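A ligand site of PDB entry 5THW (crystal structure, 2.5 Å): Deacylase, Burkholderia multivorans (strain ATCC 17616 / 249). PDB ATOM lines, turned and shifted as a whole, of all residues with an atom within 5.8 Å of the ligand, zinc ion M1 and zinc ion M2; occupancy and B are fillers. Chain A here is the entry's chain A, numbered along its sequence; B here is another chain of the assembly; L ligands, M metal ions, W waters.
Water W1 bridges ND1 of His 379 (2.6 Å) and OE2 of Glu 149 (2.8 Å).
Merely in contact with zinc ion M1: Gly 116 (3.9 Å), Glu 149 (3.7 Å) and His 379 (3.9 Å). Within 4 Å of zinc ion M1: His 104, Asp 115, Gly 116, Glu 149, His 211 and His 379. The nearest printed residue that does not touch zinc ion M1 is Gln 214 (4.3 Å).
N1 of the ligand is bound to zinc ion M1. Zinc ion M1 is bound by a ring nitrogen (NE2) of His 104 (2.3 Å). Water W1 is bound to zinc ion M1, 2.3 Å away. Zinc ion M1 is bound by NE2 of His 211, at 2.3 Å. Zinc ion M1 is bound by OD1 of Asp 115, 2.4 Å away.
Zinc ion M2 is bound by the side-chain carboxylate (OD2) of Asp 115 (2.0 Å). OE2 of Glu 150 is bound to zinc ion M2. Zinc ion M2 is bound by NE2 of His 403, at 2.1 Å. O1 of the ligand is bound to zinc ion M2, 2.3 Å away. Zinc ion M2 is bound by OE1 of Glu 150, 2.6 Å away. Slightly farther from zinc ion M2 lies a nitrogen (N1) of the ligand (2.6 Å).
NE2 of Gln 234 is in hydrogen-bond range of OH of Tyr 346 (2.8 Å). The side-chain sulfur (SD) of Met 158 sits at hydrogen-bond distance from the backbone NH (N) of His 379, 3.7 Å away. NE2 of Gln 108 lies close to OE1 of Glu 150, at 2.8 Å. The backbone NH of His 247 of chain B sits at hydrogen-bond distance from the backbone carbonyl oxygen of Ser 402 (2.9 Å). The guanidinium group (NH1) of Arg 309 sits at hydrogen-bond distance from the backbone carbonyl oxygen (O) of Gly 376 (3.3 Å). OD2 of Asp 307 is in salt-bridge range of NE of Arg 309. The side-chain amide oxygen of Asn 296 of chain B sits at hydrogen-bond distance from the side-chain amide nitrogen of Gln 108 (2.8 Å). The backbone carbonyl oxygen (O) of Gly 116 lies close to the side-chain hydroxyl (OG) of Ser 103 (3.4 Å).
O2 of the ligand lies within hydrogen-bond range of N of Gly 378 (2.6 Å). The side-chain amide nitrogen (NE2) of Gln 234 lies within hydrogen-bond range of an oxygen (O2) of the ligand (3.1 Å). OE2 of Glu 149 lies within hydrogen-bond range of N2 of the ligand, at 3.1 Å. The side-chain amide nitrogen (ND2) of Asn 296 of chain B sits at hydrogen-bond distance from an oxygen (O3) of the ligand (3.2 Å). The guanidinium group (NH1) of Arg 309 lies within salt-bridge range of an oxygen (O2) of the ligand (2.7 Å). The side-chain amide nitrogen of Gln 214 lies close to an oxygen (O1) of the ligand (3.0 Å). An oxygen (O1) of the ligand lies close to a ring nitrogen (NE2) of His 247 of chain B, 2.6 Å away. The backbone carbonyl oxygen (O) of Gly 378 is in hydrogen-bond range of a nitrogen (N2) of the ligand (3.0 Å).
Merely in contact with the ligand: Ala 377 (3.3 Å), Ala 157 (3.8 Å) and Trp 236 (3.8 Å).
Residues that only touch zinc ion M2: Gln 214. Within 4 Å of zinc ion M2: Asp 115, Glu 150, Gln 214 and His 403.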
ATOM      1  N   SER A 103     -15.626   9.060   1.980  1.00  0.00           N
ATOM      2  CA  SER A 103     -14.782   8.175   2.769  1.00  0.00           C
ATOM      3  C   SER A 103     -13.532   8.951   3.142  1.00  0.00           C
ATOM      4  O   SER A 103     -13.613  10.153   3.418  1.00  0.00           O
ATOM      5  CB  SER A 103     -14.469   6.898   1.976  1.00  0.00           C
ATOM      6  OG  SER A 103     -14.235   5.801   2.834  1.00  0.00           O
ATOM      7  N   HIS A 104     -12.377   8.302   3.134  1.00  0.00           N
ATOM      8  CA  HIS A 104     -11.138   8.960   3.492  1.00  0.00           C
ATOM      9  C   HIS A 104     -10.123   8.777   2.379  1.00  0.00           C
ATOM     10  O   HIS A 104     -10.136   7.791   1.651  1.00  0.00           O
ATOM     11  CB  HIS A 104     -10.565   8.416   4.792  1.00  0.00           C
ATOM     12  CG  HIS A 104     -10.375   6.929   4.793  1.00  0.00           C
ATOM     13  ND1 HIS A 104      -9.153   6.340   4.536  1.00  0.00           N
ATOM     14  CD2 HIS A 104     -11.242   5.920   4.994  1.00  0.00           C
ATOM     15  CE1 HIS A 104      -9.284   5.028   4.596  1.00  0.00           C
ATOM     16  NE2 HIS A 104     -10.546   4.741   4.878  1.00  0.00           N
ATOM     17  N   GLN A 108      -2.857   3.701   5.426  1.00  0.00           N
ATOM     18  CA  GLN A 108      -1.879   3.104   6.308  1.00  0.00           C
ATOM     19  C   GLN A 108      -0.469   3.224   5.710  1.00  0.00           C
ATOM     20  O   GLN A 108      -0.320   3.523   4.521  1.00  0.00           O
ATOM     21  CB  GLN A 108      -2.227   1.632   6.560  1.00  0.00           C
ATOM     22  CG  GLN A 108      -3.498   1.464   7.358  1.00  0.00           C
ATOM     23  CD  GLN A 108      -3.266   1.693   8.840  1.00  0.00           C
ATOM     24  OE1 GLN A 108      -2.145   1.589   9.330  1.00  0.00           O
ATOM     25  NE2 GLN A 108      -4.332   2.020   9.565  1.00  0.00           N
ATOM     26  N   ASP A 115      -8.614   1.069  -0.156  1.00  0.00           N
ATOM     27  CA  ASP A 115      -9.109   1.417   1.170  1.00  0.00           C
ATOM     28  C   ASP A 115      -9.364   2.925   1.257  1.00  0.00           C
ATOM     29  O   ASP A 115      -8.445   3.723   1.075  1.00  0.00           O
ATOM     30  CB  ASP A 115      -8.084   0.959   2.203  1.00  0.00           C
ATOM     31  CG  ASP A 115      -8.550   1.135   3.643  1.00  0.00           C
ATOM     32  OD1 ASP A 115      -9.679   1.604   3.888  1.00  0.00           O
ATOM     33  OD2 ASP A 115      -7.743   0.807   4.546  1.00  0.00           O
ATOM     34  N   GLY A 116     -10.618   3.301   1.519  1.00  0.00           N
ATOM     35  CA  GLY A 116     -10.980   4.701   1.652  1.00  0.00           C
ATOM     36  C   GLY A 116     -11.172   5.480   0.369  1.00  0.00           C
ATOM     37  O   GLY A 116     -12.233   6.060   0.127  1.00  0.00           O
ATOM     38  N   GLU A 149      -8.932   9.245   9.077  1.00  0.00           N
ATOM     39  CA  GLU A 149      -9.852   8.154   9.409  1.00  0.00           C
ATOM     40  C   GLU A 149      -9.108   6.935   9.912  1.00  0.00           C
ATOM     41  O   GLU A 149      -9.592   6.236  10.802  1.00  0.00           O
ATOM     42  CB  GLU A 149     -10.731   7.806   8.209  1.00  0.00           C
ATOM     43  CG  GLU A 149     -11.791   6.764   8.499  1.00  0.00           C
ATOM     44  CD  GLU A 149     -11.281   5.341   8.355  1.00  0.00           C
ATOM     45  OE1 GLU A 149     -10.201   5.155   7.735  1.00  0.00           O
ATOM     46  OE2 GLU A 149     -11.950   4.414   8.844  1.00  0.00           O
ATOM     47  N   GLU A 150      -7.917   6.669   9.364  1.00  0.00           N
ATOM     48  CA  GLU A 150      -7.178   5.443   9.683  1.00  0.00           C
ATOM     49  C   GLU A 150      -6.805   5.379  11.158  1.00  0.00           C
ATOM     50  O   GLU A 150      -6.751   4.284  11.734  1.00  0.00           O
ATOM     51  CB  GLU A 150      -5.921   5.346   8.823  1.00  0.00           C
ATOM     52  CG  GLU A 150      -6.169   4.961   7.373  1.00  0.00           C
ATOM     53  CD  GLU A 150      -6.591   3.512   7.206  1.00  0.00           C
ATOM     54  OE1 GLU A 150      -6.608   2.771   8.214  1.00  0.00           O
ATOM     55  OE2 GLU A 150      -6.920   3.117   6.065  1.00  0.00           O
ATOM     56  N   ALA A 157      -8.932   6.215  15.437  1.00  0.00           N
ATOM     57  CA  ALA A 157      -9.542   6.280  14.122  1.00  0.00           C
ATOM     58  C   ALA A 157     -10.820   7.124  14.133  1.00  0.00           C
ATOM     59  O   ALA A 157     -11.401   7.419  15.179  1.00  0.00           O
ATOM     60  CB  ALA A 157      -9.854   4.872  13.616  1.00  0.00           C
ATOM     61  N   MET A 158     -11.220   7.569  12.937  1.00  0.00           N
ATOM     62  CA  MET A 158     -12.518   8.213  12.699  1.00  0.00           C
ATOM     63  C   MET A 158     -12.727   9.445  13.572  1.00  0.00           C
ATOM     64  O   MET A 158     -13.872   9.773  13.906  1.00  0.00           O
ATOM     65  CB  MET A 158     -13.669   7.229  12.925  1.00  0.00           C
ATOM     66  CG  MET A 158     -13.662   6.025  12.017  1.00  0.00           C
ATOM     67  SD  MET A 158     -14.120   4.511  12.878  1.00  0.00           S
ATOM     68  CE  MET A 158     -15.759   4.890  13.467  1.00  0.00           C
ATOM     69  N   GLU A 209     -21.848   5.173   2.525  1.00  0.00           N
ATOM     70  CA  GLU A 209     -20.407   5.015   2.313  1.00  0.00           C
ATOM     71  C   GLU A 209     -20.119   3.737   1.542  1.00  0.00           C
ATOM     72  O   GLU A 209     -20.549   2.652   1.952  1.00  0.00           O
ATOM     73  CB  GLU A 209     -19.645   5.037   3.642  1.00  0.00           C
ATOM     74  CG  GLU A 209     -18.142   4.931   3.461  1.00  0.00           C
ATOM     75  CD  GLU A 209     -17.367   5.354   4.694  1.00  0.00           C
ATOM     76  OE1 GLU A 209     -16.133   5.201   4.708  1.00  0.00           O
ATOM     77  OE2 GLU A 209     -18.005   5.832   5.653  1.00  0.00           O
ATOM     78  N   HIS A 211     -17.314   1.053   0.185  1.00  0.00           N
ATOM     79  CA  HIS A 211     -16.028   0.591   0.707  1.00  0.00           C
ATOM     80  C   HIS A 211     -15.769  -0.853   0.281  1.00  0.00           C
ATOM     81  O   HIS A 211     -16.716  -1.597   0.023  1.00  0.00           O
ATOM     82  CB  HIS A 211     -15.991   0.694   2.247  1.00  0.00           C
ATOM     83  CG  HIS A 211     -14.618   0.899   2.809  1.00  0.00           C
ATOM     84  ND1 HIS A 211     -13.697  -0.112   2.932  1.00  0.00           N
ATOM     85  CD2 HIS A 211     -14.009   2.017   3.281  1.00  0.00           C
ATOM     86  CE1 HIS A 211     -12.583   0.366   3.448  1.00  0.00           C
ATOM     87  NE2 HIS A 211     -12.748   1.657   3.666  1.00  0.00           N
ATOM     88  N   GLN A 214     -12.594  -5.514   3.002  1.00  0.00           N
ATOM     89  CA  GLN A 214     -11.405  -5.741   3.810  1.00  0.00           C
ATOM     90  C   GLN A 214     -11.422  -7.116   4.477  1.00  0.00           C
ATOM     91  O   GLN A 214     -10.650  -7.366   5.416  1.00  0.00           O
ATOM     92  CB  GLN A 214     -11.208  -4.624   4.849  1.00  0.00           C
ATOM     93  CG  GLN A 214     -11.376  -3.231   4.234  1.00  0.00           C
ATOM     94  CD  GLN A 214     -11.201  -2.101   5.231  1.00  0.00           C
ATOM     95  OE1 GLN A 214     -12.099  -1.803   6.009  1.00  0.00           O
ATOM     96  NE2 GLN A 214     -10.039  -1.433   5.195  1.00  0.00           N
ATOM     97  N   GLN A 234     -15.654  -1.484  18.773  1.00  0.00           N
ATOM     98  CA  GLN A 234     -14.219  -1.557  18.992  1.00  0.00           C
ATOM     99  C   GLN A 234     -13.828  -0.893  20.309  1.00  0.00           C
ATOM    100  O   GLN A 234     -14.493   0.026  20.792  1.00  0.00           O
ATOM    101  CB  GLN A 234     -13.420  -0.894  17.854  1.00  0.00           C
ATOM    102  CG  GLN A 234     -13.823  -1.288  16.448  1.00  0.00           C
ATOM    103  CD  GLN A 234     -12.794  -0.855  15.422  1.00  0.00           C
ATOM    104  OE1 GLN A 234     -11.603  -0.824  15.712  1.00  0.00           O
ATOM    105  NE2 GLN A 234     -13.257  -0.483  14.237  1.00  0.00           N
ATOM    106  N   TRP A 236      -9.956   0.410  21.871  1.00  0.00           N
ATOM    107  CA  TRP A 236      -8.517   0.568  21.669  1.00  0.00           C
ATOM    108  C   TRP A 236      -7.849   1.021  22.961  1.00  0.00           C
ATOM    109  O   TRP A 236      -8.386   1.854  23.699  1.00  0.00           O
ATOM    110  CB  TRP A 236      -8.208   1.574  20.552  1.00  0.00           C
ATOM    111  CG  TRP A 236      -8.590   1.143  19.172  1.00  0.00           C
ATOM    112  CD1 TRP A 236      -9.407   0.097  18.829  1.00  0.00           C
ATOM    113  CD2 TRP A 236      -8.177   1.749  17.939  1.00  0.00           C
ATOM    114  NE1 TRP A 236      -9.518   0.020  17.466  1.00  0.00           N
ATOM    115  CE2 TRP A 236      -8.787   1.020  16.891  1.00  0.00           C
ATOM    116  CE3 TRP A 236      -7.370   2.849  17.621  1.00  0.00           C
ATOM    117  CZ2 TRP A 236      -8.592   1.355  15.547  1.00  0.00           C
ATOM    118  CZ3 TRP A 236      -7.183   3.168  16.290  1.00  0.00           C
ATOM    119  CH2 TRP A 236      -7.788   2.425  15.273  1.00  0.00           C
ATOM    120  N   ASP A 307      -5.978  -3.691  20.298  1.00  0.00           N
ATOM    121  CA  ASP A 307      -7.115  -3.515  19.405  1.00  0.00           C
ATOM    122  C   ASP A 307      -8.086  -4.664  19.689  1.00  0.00           C
ATOM    123  O   ASP A 307      -7.753  -5.836  19.459  1.00  0.00           O
ATOM    124  CB  ASP A 307      -6.644  -3.529  17.948  1.00  0.00           C
ATOM    125  CG  ASP A 307      -7.776  -3.303  16.930  1.00  0.00           C
ATOM    126  OD1 ASP A 307      -7.647  -2.374  16.097  1.00  0.00           O
ATOM    127  OD2 ASP A 307      -8.786  -4.048  16.951  1.00  0.00           O
ATOM    128  N   ARG A 309     -12.134  -6.028  19.020  1.00  0.00           N
ATOM    129  CA  ARG A 309     -13.342  -5.846  18.228  1.00  0.00           C
ATOM    130  C   ARG A 309     -14.282  -7.019  18.441  1.00  0.00           C
ATOM    131  O   ARG A 309     -13.834  -8.154  18.599  1.00  0.00           O
ATOM    132  CB  ARG A 309     -13.040  -5.701  16.734  1.00  0.00           C
ATOM    133  CG  ARG A 309     -12.037  -4.616  16.419  1.00  0.00           C
ATOM    134  CD  ARG A 309     -11.758  -4.463  14.945  1.00  0.00           C
ATOM    135  NE  ARG A 309     -10.550  -3.677  14.749  1.00  0.00           N
ATOM    136  CZ  ARG A 309     -10.347  -2.847  13.738  1.00  0.00           C
ATOM    137  NH1 ARG A 309     -11.286  -2.676  12.809  1.00  0.00           N
ATOM    138  NH2 ARG A 309      -9.199  -2.181  13.646  1.00  0.00           N
ATOM    139  N   TYR A 346     -16.535   2.542  20.814  1.00  0.00           N
ATOM    140  CA  TYR A 346     -17.848   2.798  20.250  1.00  0.00           C
ATOM    141  C   TYR A 346     -18.624   1.491  20.159  1.00  0.00           C
ATOM    142  O   TYR A 346     -18.067   0.459  19.784  1.00  0.00           O
ATOM    143  CB  TYR A 346     -17.791   3.512  18.885  1.00  0.00           C
ATOM    144  CG  TYR A 346     -17.253   2.710  17.720  1.00  0.00           C
ATOM    145  CD1 TYR A 346     -15.914   2.808  17.356  1.00  0.00           C
ATOM    146  CD2 TYR A 346     -18.094   1.927  16.940  1.00  0.00           C
ATOM    147  CE1 TYR A 346     -15.425   2.111  16.284  1.00  0.00           C
ATOM    148  CE2 TYR A 346     -17.608   1.227  15.855  1.00  0.00           C
ATOM    149  CZ  TYR A 346     -16.273   1.327  15.537  1.00  0.00           C
ATOM    150  OH  TYR A 346     -15.769   0.637  14.460  1.00  0.00           O
ATOM    151  N   GLY A 376     -16.399  -5.411   9.434  1.00  0.00           N
ATOM    152  CA  GLY A 376     -15.351  -5.728  10.383  1.00  0.00           C
ATOM    153  C   GLY A 376     -14.499  -4.552  10.799  1.00  0.00           C
ATOM    154  O   GLY A 376     -13.826  -4.617  11.835  1.00  0.00           O
ATOM    155  N   ALA A 377     -14.518  -3.471  10.030  1.00  0.00           N
ATOM    156  CA  ALA A 377     -13.731  -2.289  10.319  1.00  0.00           C
ATOM    157  C   ALA A 377     -14.648  -1.128  10.648  1.00  0.00           C
ATOM    158  O   ALA A 377     -15.859  -1.163  10.371  1.00  0.00           O
ATOM    159  CB  ALA A 377     -12.818  -1.903   9.140  1.00  0.00           C
ATOM    160  N   GLY A 378     -14.065  -0.097  11.244  1.00  0.00           N
ATOM    161  CA  GLY A 378     -14.793   1.110  11.526  1.00  0.00           C
ATOM    162  C   GLY A 378     -14.705   2.028  10.317  1.00  0.00           C
ATOM    163  O   GLY A 378     -13.706   2.058   9.609  1.00  0.00           O
ATOM    164  N   HIS A 379     -15.785   2.768  10.081  1.00  0.00           N
ATOM    165  CA  HIS A 379     -15.811   3.699   8.980  1.00  0.00           C
ATOM    166  C   HIS A 379     -16.462   4.975   9.481  1.00  0.00           C
ATOM    167  O   HIS A 379     -17.131   4.986  10.512  1.00  0.00           O
ATOM    168  CB  HIS A 379     -16.567   3.116   7.779  1.00  0.00           C
ATOM    169  CG  HIS A 379     -16.082   1.759   7.364  1.00  0.00           C
ATOM    170  ND1 HIS A 379     -14.891   1.556   6.696  1.00  0.00           N
ATOM    171  CD2 HIS A 379     -16.630   0.532   7.531  1.00  0.00           C
ATOM    172  CE1 HIS A 379     -14.726   0.264   6.478  1.00  0.00           C
ATOM    173  NE2 HIS A 379     -15.775  -0.382   6.967  1.00  0.00           N
ATOM    174  N   SER A 402      -6.641  -6.448   3.342  1.00  0.00           N
ATOM    175  CA  SER A 402      -6.547  -4.996   3.356  1.00  0.00           C
ATOM    176  C   SER A 402      -5.480  -4.616   4.379  1.00  0.00           C
ATOM    177  O   SER A 402      -5.029  -5.445   5.178  1.00  0.00           O
ATOM    178  CB  SER A 402      -7.875  -4.320   3.689  1.00  0.00           C
ATOM    179  OG  SER A 402      -7.798  -2.904   3.558  1.00  0.00           O
ATOM    180  N   HIS A 403      -5.071  -3.345   4.344  1.00  0.00           N
ATOM    181  CA  HIS A 403      -3.905  -2.873   5.101  1.00  0.00           C
ATOM    182  C   HIS A 403      -2.651  -3.655   4.723  1.00  0.00           C
ATOM    183  O   HIS A 403      -1.752  -3.870   5.546  1.00  0.00           O
ATOM    184  CB  HIS A 403      -4.141  -2.895   6.616  1.00  0.00           C
ATOM    185  CG  HIS A 403      -5.083  -1.828   7.086  1.00  0.00           C
ATOM    186  ND1 HIS A 403      -5.459  -1.688   8.398  1.00  0.00           N
ATOM    187  CD2 HIS A 403      -5.713  -0.840   6.403  1.00  0.00           C
ATOM    188  CE1 HIS A 403      -6.280  -0.659   8.514  1.00  0.00           C
ATOM    189  NE2 HIS A 403      -6.448  -0.130   7.319  1.00  0.00           N
ATOM    190  N   HIS B 247      -5.149  -6.287   7.908  1.00  0.00           N
ATOM    191  CA  HIS B 247      -6.025  -5.444   8.704  1.00  0.00           C
ATOM    192  C   HIS B 247      -6.300  -6.089  10.058  1.00  0.00           C
ATOM    193  O   HIS B 247      -6.576  -7.293  10.140  1.00  0.00           O
ATOM    194  CB  HIS B 247      -7.343  -5.210   7.974  1.00  0.00           C
ATOM    195  CG  HIS B 247      -8.075  -3.980   8.417  1.00  0.00           C
ATOM    196  ND1 HIS B 247      -8.483  -3.775   9.723  1.00  0.00           N
ATOM    197  CD2 HIS B 247      -8.470  -2.879   7.728  1.00  0.00           C
ATOM    198  CE1 HIS B 247      -9.089  -2.611   9.825  1.00  0.00           C
ATOM    199  NE2 HIS B 247      -9.090  -2.045   8.622  1.00  0.00           N
ATOM    200  N   ASN B 296      -3.477  -0.594  14.125  1.00  0.00           N
ATOM    201  CA  ASN B 296      -4.516  -1.403  13.502  1.00  0.00           C
ATOM    202  C   ASN B 296      -4.014  -2.163  12.277  1.00  0.00           C
ATOM    203  O   ASN B 296      -4.769  -2.428  11.332  1.00  0.00           O
ATOM    204  CB  ASN B 296      -5.748  -0.549  13.183  1.00  0.00           C
ATOM    205  CG  ASN B 296      -5.432   0.691  12.355  1.00  0.00           C
ATOM    206  OD1 ASN B 296      -4.276   1.119  12.240  1.00  0.00           O
ATOM    207  ND2 ASN B 296      -6.464   1.311  11.811  1.00  0.00           N
HETATM  208  O1  LIG L   1      -9.641   0.297   7.576  1.00  0.00           O
HETATM  209  C1  LIG L   1     -10.221   1.343   7.796  1.00  0.00           C
HETATM  210  N1  LIG L   1     -10.263   2.308   6.895  1.00  0.00           N
HETATM  211  N2  LIG L   1     -10.819   1.560   8.970  1.00  0.00           N
HETATM  212  C2  LIG L   1     -10.100   2.201  10.055  1.00  0.00           C
HETATM  213  C3  LIG L   1     -10.765   1.951  11.400  1.00  0.00           C
HETATM  214  C4  LIG L   1     -10.554   0.497  11.732  1.00  0.00           C
HETATM  215  O2  LIG L   1     -11.548  -0.278  11.688  1.00  0.00           O
HETATM  216  O3  LIG L   1      -9.402   0.112  12.046  1.00  0.00           O
HETATM  217 ZN    ZN M   1     -11.378   2.655   5.282  1.00  0.00          ZN
HETATM  218 ZN    ZN M   2      -7.873   1.259   6.523  1.00  0.00          ZN
HETATM  219  O   HOH W   1     -13.176   3.557   6.422  1.00  0.00           O
